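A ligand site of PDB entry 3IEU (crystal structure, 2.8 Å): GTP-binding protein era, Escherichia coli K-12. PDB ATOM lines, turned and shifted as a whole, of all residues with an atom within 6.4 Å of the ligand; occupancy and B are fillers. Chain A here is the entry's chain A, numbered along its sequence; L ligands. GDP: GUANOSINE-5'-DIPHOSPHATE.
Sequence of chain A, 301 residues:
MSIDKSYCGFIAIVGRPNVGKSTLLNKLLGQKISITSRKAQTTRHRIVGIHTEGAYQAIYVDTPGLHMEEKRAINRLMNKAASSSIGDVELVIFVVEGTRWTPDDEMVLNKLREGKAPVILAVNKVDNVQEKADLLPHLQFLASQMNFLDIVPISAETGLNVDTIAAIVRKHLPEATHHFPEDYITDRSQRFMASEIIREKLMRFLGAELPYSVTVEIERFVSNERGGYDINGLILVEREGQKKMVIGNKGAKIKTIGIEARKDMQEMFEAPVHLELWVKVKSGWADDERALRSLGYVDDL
N of Ser 22 sits at hydrogen-bond distance from O2A of the ligand.
An oxygen (O3B) of the ligand is in hydrogen-bond range of the side-chain hydroxyl (OG) of Ser 22 (2.5 Å).
The side-chain carboxylate (OD1) of Asp 127 is in hydrogen-bond range of a nitrogen (N1) of the ligand (2.7 Å).
The backbone NH of Lys 21 sits at hydrogen-bond distance from an oxygen (O1B) of the ligand (2.8 Å).
The side-chain amino group (NZ) of Lys 21 is in salt-bridge range of an oxygen (O1B) of the ligand, at 3.1 Å.
O4' of the ligand is in hydrogen-bond range of NZ of Lys 125 (2.8 Å).
The backbone NH (N) of Ala 156 is in hydrogen-bond range of an oxygen (O6) of the ligand, at 2.8 Å.
An oxygen (O2A) of the ligand is in hydrogen-bond range of the backbone NH (N) of Thr 23 (2.9 Å).
The side-chain hydroxyl (OG1) of Thr 23 lies within hydrogen-bond range of an oxygen (O2A) of the ligand (2.9 Å).
O6 of the ligand sits at hydrogen-bond distance from OG of Ser 155.
The backbone NH (N) of Asn 18 sits at hydrogen-bond distance from an oxygen (O2B) of the ligand.
The backbone NH (N) of Gly 20 is in hydrogen-bond range of an oxygen (O1B) of the ligand (3.0 Å).
ND2 of Asn 124 lies within hydrogen-bond range of N7 of the ligand (3.0 Å).
N of Glu 157 lies within hydrogen-bond range of O6 of the ligand.
N of Val 19 sits at hydrogen-bond distance from O1B of the ligand, 3.5 Å away.
OD1 of Asp 127 is in hydrogen-bond range of OG of Ser 155 (3.4 Å).
The side-chain amino group (NZ) of Lys 21 lies within hydrogen-bond range of the backbone carbonyl oxygen (O) of Gly 15 (2.6 Å).
The side-chain amino group of Lys 125 lies within hydrogen-bond range of the backbone carbonyl oxygen of Asn 18 (3.1 Å).
The backbone NH (N) of Lys 125 lies within hydrogen-bond range of the backbone carbonyl oxygen (O) of Ile 154 (3.3 Å).
N of Ala 156 sits at hydrogen-bond distance from OD1 of Asn 124.
The side-chain hydroxyl (OG) of Ser 155 lies close to the backbone NH (N) of Glu 157 (3.5 Å).
The side-chain hydroxyl of Thr 158 lies within hydrogen-bond range of the side-chain hydroxyl of Ser 155.
ND2 of Asn 124 sits at hydrogen-bond distance from O of Val 19, at 2.7 Å.
Pro 17 touches the ligand (CA to O2B, 3.8 Å).
Asn 128 touches the ligand (OD1 to N2, 3.7 Å).
14 residues have an atom within 4 Å of the ligand: Pro 17, Asn 18, Val 19, Gly 20, Lys 21, Ser 22, Thr 23, Asn 124, Lys 125, Asp 127, Asn 128, Ser 155, Ala 156 and Glu 157.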
ATOM      1  N   GLY A  15      -5.344  33.497 -12.055  1.00  0.00           N
ATOM      2  CA  GLY A  15      -3.925  33.347 -11.851  1.00  0.00           C
ATOM      3  C   GLY A  15      -3.247  32.797 -13.086  1.00  0.00           C
ATOM      4  O   GLY A  15      -3.828  31.971 -13.793  1.00  0.00           O
ATOM      5  N   ARG A  16      -2.026  33.245 -13.349  1.00  0.00           N
ATOM      6  CA  ARG A  16      -1.280  32.816 -14.518  1.00  0.00           C
ATOM      7  C   ARG A  16      -1.165  31.289 -14.612  1.00  0.00           C
ATOM      8  O   ARG A  16      -1.319  30.586 -13.604  1.00  0.00           O
ATOM      9  CB  ARG A  16       0.115  33.446 -14.520  1.00  0.00           C
ATOM     10  CG  ARG A  16       1.061  32.813 -13.534  1.00  0.00           C
ATOM     11  CD  ARG A  16       2.527  33.251 -13.673  1.00  0.00           C
ATOM     12  NE  ARG A  16       3.261  32.725 -12.524  1.00  0.00           N
ATOM     13  CZ  ARG A  16       3.780  31.508 -12.461  1.00  0.00           C
ATOM     14  NH1 ARG A  16       3.677  30.674 -13.485  1.00  0.00           N
ATOM     15  NH2 ARG A  16       4.395  31.114 -11.359  1.00  0.00           N
ATOM     16  N   PRO A  17      -0.902  30.776 -15.830  1.00  0.00           N
ATOM     17  CA  PRO A  17      -0.801  29.326 -16.080  1.00  0.00           C
ATOM     18  C   PRO A  17       0.212  28.622 -15.177  1.00  0.00           C
ATOM     19  O   PRO A  17       1.333  29.090 -14.959  1.00  0.00           O
ATOM     20  CB  PRO A  17      -0.361  29.256 -17.546  1.00  0.00           C
ATOM     21  CG  PRO A  17      -0.886  30.517 -18.147  1.00  0.00           C
ATOM     22  CD  PRO A  17      -0.781  31.550 -17.072  1.00  0.00           C
ATOM     23  N   ASN A  18      -0.225  27.497 -14.634  1.00  0.00           N
ATOM     24  CA  ASN A  18       0.613  26.560 -13.887  1.00  0.00           C
ATOM     25  C   ASN A  18       0.666  26.706 -12.400  1.00  0.00           C
ATOM     26  O   ASN A  18       1.338  25.928 -11.725  1.00  0.00           O
ATOM     27  CB  ASN A  18       2.021  26.440 -14.458  1.00  0.00           C
ATOM     28  CG  ASN A  18       2.244  25.087 -15.077  1.00  0.00           C
ATOM     29  OD1 ASN A  18       1.675  24.769 -16.137  1.00  0.00           O
ATOM     30  ND2 ASN A  18       3.028  24.241 -14.386  1.00  0.00           N
ATOM     31  N   VAL A  19      -0.052  27.691 -11.886  1.00  0.00           N
ATOM     32  CA  VAL A  19      -0.039  27.955 -10.454  1.00  0.00           C
ATOM     33  C   VAL A  19      -0.879  26.913  -9.706  1.00  0.00           C
ATOM     34  O   VAL A  19      -0.768  26.769  -8.492  1.00  0.00           O
ATOM     35  CB  VAL A  19      -0.529  29.377 -10.147  1.00  0.00           C
ATOM     36  CG1 VAL A  19       0.216  30.384 -11.012  1.00  0.00           C
ATOM     37  CG2 VAL A  19      -2.025  29.502 -10.374  1.00  0.00           C
ATOM     38  N   GLY A  20      -1.720  26.176 -10.440  1.00  0.00           N
ATOM     39  CA  GLY A  20      -2.528  25.109  -9.845  1.00  0.00           C
ATOM     40  C   GLY A  20      -4.021  25.387  -9.725  1.00  0.00           C
ATOM     41  O   GLY A  20      -4.699  24.756  -8.898  1.00  0.00           O
ATOM     42  N   LYS A  21      -4.527  26.303 -10.549  1.00  0.00           N
ATOM     43  CA  LYS A  21      -5.962  26.606 -10.612  1.00  0.00           C
ATOM     44  C   LYS A  21      -6.837  25.363 -10.803  1.00  0.00           C
ATOM     45  O   LYS A  21      -7.758  25.126 -10.037  1.00  0.00           O
ATOM     46  CB  LYS A  21      -6.234  27.606 -11.733  1.00  0.00           C
ATOM     47  CG  LYS A  21      -5.510  28.942 -11.593  1.00  0.00           C
ATOM     48  CD  LYS A  21      -5.875  29.941 -12.696  1.00  0.00           C
ATOM     49  CE  LYS A  21      -5.526  29.441 -14.110  1.00  0.00           C
ATOM     50  NZ  LYS A  21      -4.097  29.421 -14.449  1.00  0.00           N
ATOM     51  N   SER A  22      -6.558  24.565 -11.827  1.00  0.00           N
ATOM     52  CA  SER A  22      -7.411  23.407 -12.102  1.00  0.00           C
ATOM     53  C   SER A  22      -7.292  22.383 -10.992  1.00  0.00           C
ATOM     54  O   SER A  22      -8.258  21.687 -10.668  1.00  0.00           O
ATOM     55  CB  SER A  22      -7.051  22.772 -13.445  1.00  0.00           C
ATOM     56  OG  SER A  22      -6.750  23.790 -14.402  1.00  0.00           O
ATOM     57  N   THR A  23      -6.116  22.309 -10.381  1.00  0.00           N
ATOM     58  CA  THR A  23      -5.884  21.338  -9.333  1.00  0.00           C
ATOM     59  C   THR A  23      -6.723  21.680  -8.108  1.00  0.00           C
ATOM     60  O   THR A  23      -7.276  20.791  -7.450  1.00  0.00           O
ATOM     61  CB  THR A  23      -4.423  21.307  -8.900  1.00  0.00           C
ATOM     62  OG1 THR A  23      -3.584  21.193 -10.052  1.00  0.00           O
ATOM     63  CG2 THR A  23      -4.196  20.165  -7.935  1.00  0.00           C
ATOM     64  N   LEU A  24      -6.823  22.965  -7.828  1.00  0.00           N
ATOM     65  CA  LEU A  24      -7.576  23.459  -6.690  1.00  0.00           C
ATOM     66  C   LEU A  24      -9.076  23.385  -6.968  1.00  0.00           C
ATOM     67  O   LEU A  24      -9.873  23.010  -6.104  1.00  0.00           O
ATOM     68  CB  LEU A  24      -7.171  24.898  -6.417  1.00  0.00           C
ATOM     69  CG  LEU A  24      -8.162  25.713  -5.607  1.00  0.00           C
ATOM     70  CD1 LEU A  24      -8.225  25.200  -4.178  1.00  0.00           C
ATOM     71  CD2 LEU A  24      -7.799  27.177  -5.688  1.00  0.00           C
ATOM     72  N   THR A  36      -8.637  15.962 -15.536  1.00  0.00           N
ATOM     73  CA  THR A  36      -7.810  17.072 -15.985  1.00  0.00           C
ATOM     74  C   THR A  36      -7.644  17.080 -17.507  1.00  0.00           C
ATOM     75  O   THR A  36      -8.002  16.128 -18.202  1.00  0.00           O
ATOM     76  CB  THR A  36      -6.424  17.064 -15.324  1.00  0.00           C
ATOM     77  OG1 THR A  36      -5.660  15.977 -15.836  1.00  0.00           O
ATOM     78  CG2 THR A  36      -6.560  16.947 -13.811  1.00  0.00           C
ATOM     79  N   ARG A  38      -4.669  18.735 -20.126  1.00  0.00           N
ATOM     80  CA  ARG A  38      -3.450  19.511 -20.358  1.00  0.00           C
ATOM     81  C   ARG A  38      -3.589  20.414 -21.597  1.00  0.00           C
ATOM     82  O   ARG A  38      -2.617  21.051 -22.018  1.00  0.00           O
ATOM     83  CB  ARG A  38      -2.216  18.590 -20.496  1.00  0.00           C
ATOM     84  CG  ARG A  38      -1.990  17.610 -19.325  1.00  0.00           C
ATOM     85  CD  ARG A  38      -0.848  18.006 -18.372  1.00  0.00           C
ATOM     86  NE  ARG A  38      -0.315  16.835 -17.658  1.00  0.00           N
ATOM     87  CZ  ARG A  38       0.838  16.788 -16.997  1.00  0.00           C
ATOM     88  NH1 ARG A  38       1.619  17.863 -16.933  1.00  0.00           N
ATOM     89  NH2 ARG A  38       1.231  15.664 -16.392  1.00  0.00           N
ATOM     90  N   ALA A  40      -6.380  22.727 -21.788  1.00  0.00           N
ATOM     91  CA  ALA A  40      -6.908  23.968 -21.226  1.00  0.00           C
ATOM     92  C   ALA A  40      -7.281  25.003 -22.304  1.00  0.00           C
ATOM     93  O   ALA A  40      -6.415  25.733 -22.784  1.00  0.00           O
ATOM     94  CB  ALA A  40      -5.901  24.565 -20.233  1.00  0.00           C
ATOM     95  N   VAL A  95      -4.716  33.052  -7.476  1.00  0.00           N
ATOM     96  CA  VAL A  95      -3.846  31.940  -7.146  1.00  0.00           C
ATOM     97  C   VAL A  95      -2.437  32.239  -7.640  1.00  0.00           C
ATOM     98  O   VAL A  95      -2.262  32.713  -8.767  1.00  0.00           O
ATOM     99  CB  VAL A  95      -4.354  30.626  -7.771  1.00  0.00           C
ATOM    100  CG1 VAL A  95      -3.478  29.450  -7.356  1.00  0.00           C
ATOM    101  CG2 VAL A  95      -5.768  30.371  -7.350  1.00  0.00           C
ATOM    102  N   ASN A 124      -0.396  28.850  -3.500  1.00  0.00           N
ATOM    103  CA  ASN A 124      -0.347  27.426  -3.750  1.00  0.00           C
ATOM    104  C   ASN A 124       1.083  26.883  -3.797  1.00  0.00           C
ATOM    105  O   ASN A 124       2.038  27.649  -3.738  1.00  0.00           O
ATOM    106  CB  ASN A 124      -1.103  27.107  -5.040  1.00  0.00           C
ATOM    107  CG  ASN A 124      -1.419  25.628  -5.192  1.00  0.00           C
ATOM    108  OD1 ASN A 124      -1.748  24.939  -4.225  1.00  0.00           O
ATOM    109  ND2 ASN A 124      -1.312  25.134  -6.426  1.00  0.00           N
ATOM    110  N   LYS A 125       1.200  25.558  -3.878  1.00  0.00           N
ATOM    111  CA  LYS A 125       2.483  24.888  -4.026  1.00  0.00           C
ATOM    112  C   LYS A 125       3.356  25.178  -2.821  1.00  0.00           C
ATOM    113  O   LYS A 125       4.580  25.237  -2.897  1.00  0.00           O
ATOM    114  CB  LYS A 125       3.168  25.307  -5.321  1.00  0.00           C
ATOM    115  CG  LYS A 125       2.348  25.005  -6.555  1.00  0.00           C
ATOM    116  CD  LYS A 125       3.205  24.804  -7.783  1.00  0.00           C
ATOM    117  CE  LYS A 125       2.336  24.588  -9.021  1.00  0.00           C
ATOM    118  NZ  LYS A 125       3.044  23.855 -10.111  1.00  0.00           N
ATOM    119  N   VAL A 126       2.683  25.370  -1.691  1.00  0.00           N
ATOM    120  CA  VAL A 126       3.354  25.660  -0.429  1.00  0.00           C
ATOM    121  C   VAL A 126       4.202  24.478   0.010  1.00  0.00           C
ATOM    122  O   VAL A 126       5.297  24.660   0.551  1.00  0.00           O
ATOM    123  CB  VAL A 126       2.335  26.055   0.663  1.00  0.00           C
ATOM    124  CG1 VAL A 126       2.508  25.226   1.920  1.00  0.00           C
ATOM    125  CG2 VAL A 126       2.440  27.519   0.949  1.00  0.00           C
ATOM    126  N   ASP A 127       3.720  23.274  -0.253  1.00  0.00           N
ATOM    127  CA  ASP A 127       4.472  22.060   0.031  1.00  0.00           C
ATOM    128  C   ASP A 127       5.815  22.073  -0.698  1.00  0.00           C
ATOM    129  O   ASP A 127       6.800  21.466  -0.248  1.00  0.00           O
ATOM    130  CB  ASP A 127       3.659  20.827  -0.393  1.00  0.00           C
ATOM    131  CG  ASP A 127       3.339  20.811  -1.890  1.00  0.00           C
ATOM    132  OD1 ASP A 127       2.837  21.831  -2.406  1.00  0.00           O
ATOM    133  OD2 ASP A 127       3.597  19.795  -2.551  1.00  0.00           O
ATOM    134  N   ASN A 128       5.863  22.784  -1.819  1.00  0.00           N
ATOM    135  CA  ASN A 128       7.003  22.761  -2.734  1.00  0.00           C
ATOM    136  C   ASN A 128       8.006  23.887  -2.481  1.00  0.00           C
ATOM    137  O   ASN A 128       8.882  24.160  -3.316  1.00  0.00           O
ATOM    138  CB  ASN A 128       6.495  22.850  -4.167  1.00  0.00           C
ATOM    139  CG  ASN A 128       7.398  22.158  -5.151  1.00  0.00           C
ATOM    140  OD1 ASN A 128       7.080  22.060  -6.329  1.00  0.00           O
ATOM    141  ND2 ASN A 128       8.549  21.683  -4.667  1.00  0.00           N
ATOM    142  N   ILE A 154      -1.707  27.252   0.638  1.00  0.00           N
ATOM    143  CA  ILE A 154      -2.319  25.944   0.456  1.00  0.00           C
ATOM    144  C   ILE A 154      -1.455  25.025  -0.351  1.00  0.00           C
ATOM    145  O   ILE A 154      -0.505  25.439  -1.034  1.00  0.00           O
ATOM    146  CB  ILE A 154      -3.634  26.043  -0.359  1.00  0.00           C
ATOM    147  CG1 ILE A 154      -3.355  26.614  -1.741  1.00  0.00           C
ATOM    148  CG2 ILE A 154      -4.670  26.889   0.365  1.00  0.00           C
ATOM    149  CD1 ILE A 154      -4.509  26.550  -2.690  1.00  0.00           C
ATOM    150  N   SER A 155      -1.809  23.755  -0.314  1.00  0.00           N
ATOM    151  CA  SER A 155      -1.325  22.833  -1.305  1.00  0.00           C
ATOM    152  C   SER A 155      -2.531  22.182  -1.977  1.00  0.00           C
ATOM    153  O   SER A 155      -3.241  21.393  -1.365  1.00  0.00           O
ATOM    154  CB  SER A 155      -0.473  21.752  -0.666  1.00  0.00           C
ATOM    155  OG  SER A 155      -0.253  20.701  -1.578  1.00  0.00           O
ATOM    156  N   ALA A 156      -2.773  22.526  -3.229  1.00  0.00           N
ATOM    157  CA  ALA A 156      -3.914  21.957  -3.932  1.00  0.00           C
ATOM    158  C   ALA A 156      -3.782  20.448  -4.006  1.00  0.00           C
ATOM    159  O   ALA A 156      -4.775  19.728  -3.936  1.00  0.00           O
ATOM    160  CB  ALA A 156      -4.037  22.545  -5.319  1.00  0.00           C
ATOM    161  N   GLU A 157      -2.539  19.982  -4.102  1.00  0.00           N
ATOM    162  CA  GLU A 157      -2.214  18.542  -4.194  1.00  0.00           C
ATOM    163  C   GLU A 157      -2.586  17.761  -2.932  1.00  0.00           C
ATOM    164  O   GLU A 157      -3.257  16.715  -2.984  1.00  0.00           O
ATOM    165  CB  GLU A 157      -0.719  18.398  -4.474  1.00  0.00           C
ATOM    166  CG  GLU A 157      -0.349  17.177  -5.265  1.00  0.00           C
ATOM    167  CD  GLU A 157       1.122  17.171  -5.618  1.00  0.00           C
ATOM    168  OE1 GLU A 157       1.947  16.819  -4.735  1.00  0.00           O
ATOM    169  OE2 GLU A 157       1.465  17.507  -6.776  1.00  0.00           O
ATOM    170  N   THR A 158      -2.151  18.287  -1.787  1.00  0.00           N
ATOM    171  CA  THR A 158      -2.360  17.686  -0.481  1.00  0.00           C
ATOM    172  C   THR A 158      -3.763  17.909   0.054  1.00  0.00           C
ATOM    173  O   THR A 158      -4.309  17.079   0.774  1.00  0.00           O
ATOM    174  CB  THR A 158      -1.459  18.336   0.566  1.00  0.00           C
ATOM    175  OG1 THR A 158      -0.100  18.297   0.119  1.00  0.00           O
ATOM    176  CG2 THR A 158      -1.585  17.632   1.915  1.00  0.00           C
HETATM  177  PB  GDP L   1      -3.285  25.765 -13.935  1.00  0.00           P
HETATM  178  O1B GDP L   1      -3.261  26.898 -12.919  1.00  0.00           O
HETATM  179  O2B GDP L   1      -2.815  26.259 -15.293  1.00  0.00           O
HETATM  180  O3B GDP L   1      -4.704  25.258 -14.032  1.00  0.00           O
HETATM  181  O3A GDP L   1      -2.299  24.617 -13.417  1.00  0.00           O
HETATM  182  PA  GDP L   1      -2.733  23.212 -12.774  1.00  0.00           P
HETATM  183  O1A GDP L   1      -2.975  22.221 -13.907  1.00  0.00           O
HETATM  184  O2A GDP L   1      -3.914  23.374 -11.872  1.00  0.00           O
HETATM  185  O5' GDP L   1      -1.419  22.726 -11.985  1.00  0.00           O
HETATM  186  C5' GDP L   1      -0.263  22.523 -12.809  1.00  0.00           C
HETATM  187  C4' GDP L   1       0.756  21.642 -12.162  1.00  0.00           C
HETATM  188  O4' GDP L   1       0.939  22.130 -10.850  1.00  0.00           O
HETATM  189  C3' GDP L   1       0.227  20.224 -12.029  1.00  0.00           C
HETATM  190  O3' GDP L   1       1.244  19.303 -12.395  1.00  0.00           O
HETATM  191  C2' GDP L   1      -0.085  20.068 -10.559  1.00  0.00           C
HETATM  192  O2' GDP L   1       0.089  18.736 -10.066  1.00  0.00           O
HETATM  193  C1' GDP L   1       0.904  21.032  -9.934  1.00  0.00           C
HETATM  194  N9  GDP L   1       0.377  21.421  -8.622  1.00  0.00           N
HETATM  195  C8  GDP L   1      -0.844  21.946  -8.379  1.00  0.00           C
HETATM  196  N7  GDP L   1      -1.005  22.169  -7.045  1.00  0.00           N
HETATM  197  C5  GDP L   1       0.124  21.796  -6.435  1.00  0.00           C
HETATM  198  C6  GDP L   1       0.611  21.765  -5.045  1.00  0.00           C
HETATM  199  O6  GDP L   1      -0.116  22.187  -4.113  1.00  0.00           O
HETATM  200  N1  GDP L   1       1.849  21.296  -4.827  1.00  0.00           N
HETATM  201  C2  GDP L   1       2.637  20.846  -5.824  1.00  0.00           C
HETATM  202  N2  GDP L   1       3.879  20.392  -5.514  1.00  0.00           N
HETATM  203  N3  GDP L   1       2.259  20.841  -7.124  1.00  0.00           N
HETATM  204  C4  GDP L   1       1.030  21.294  -7.469  1.00  0.00           C
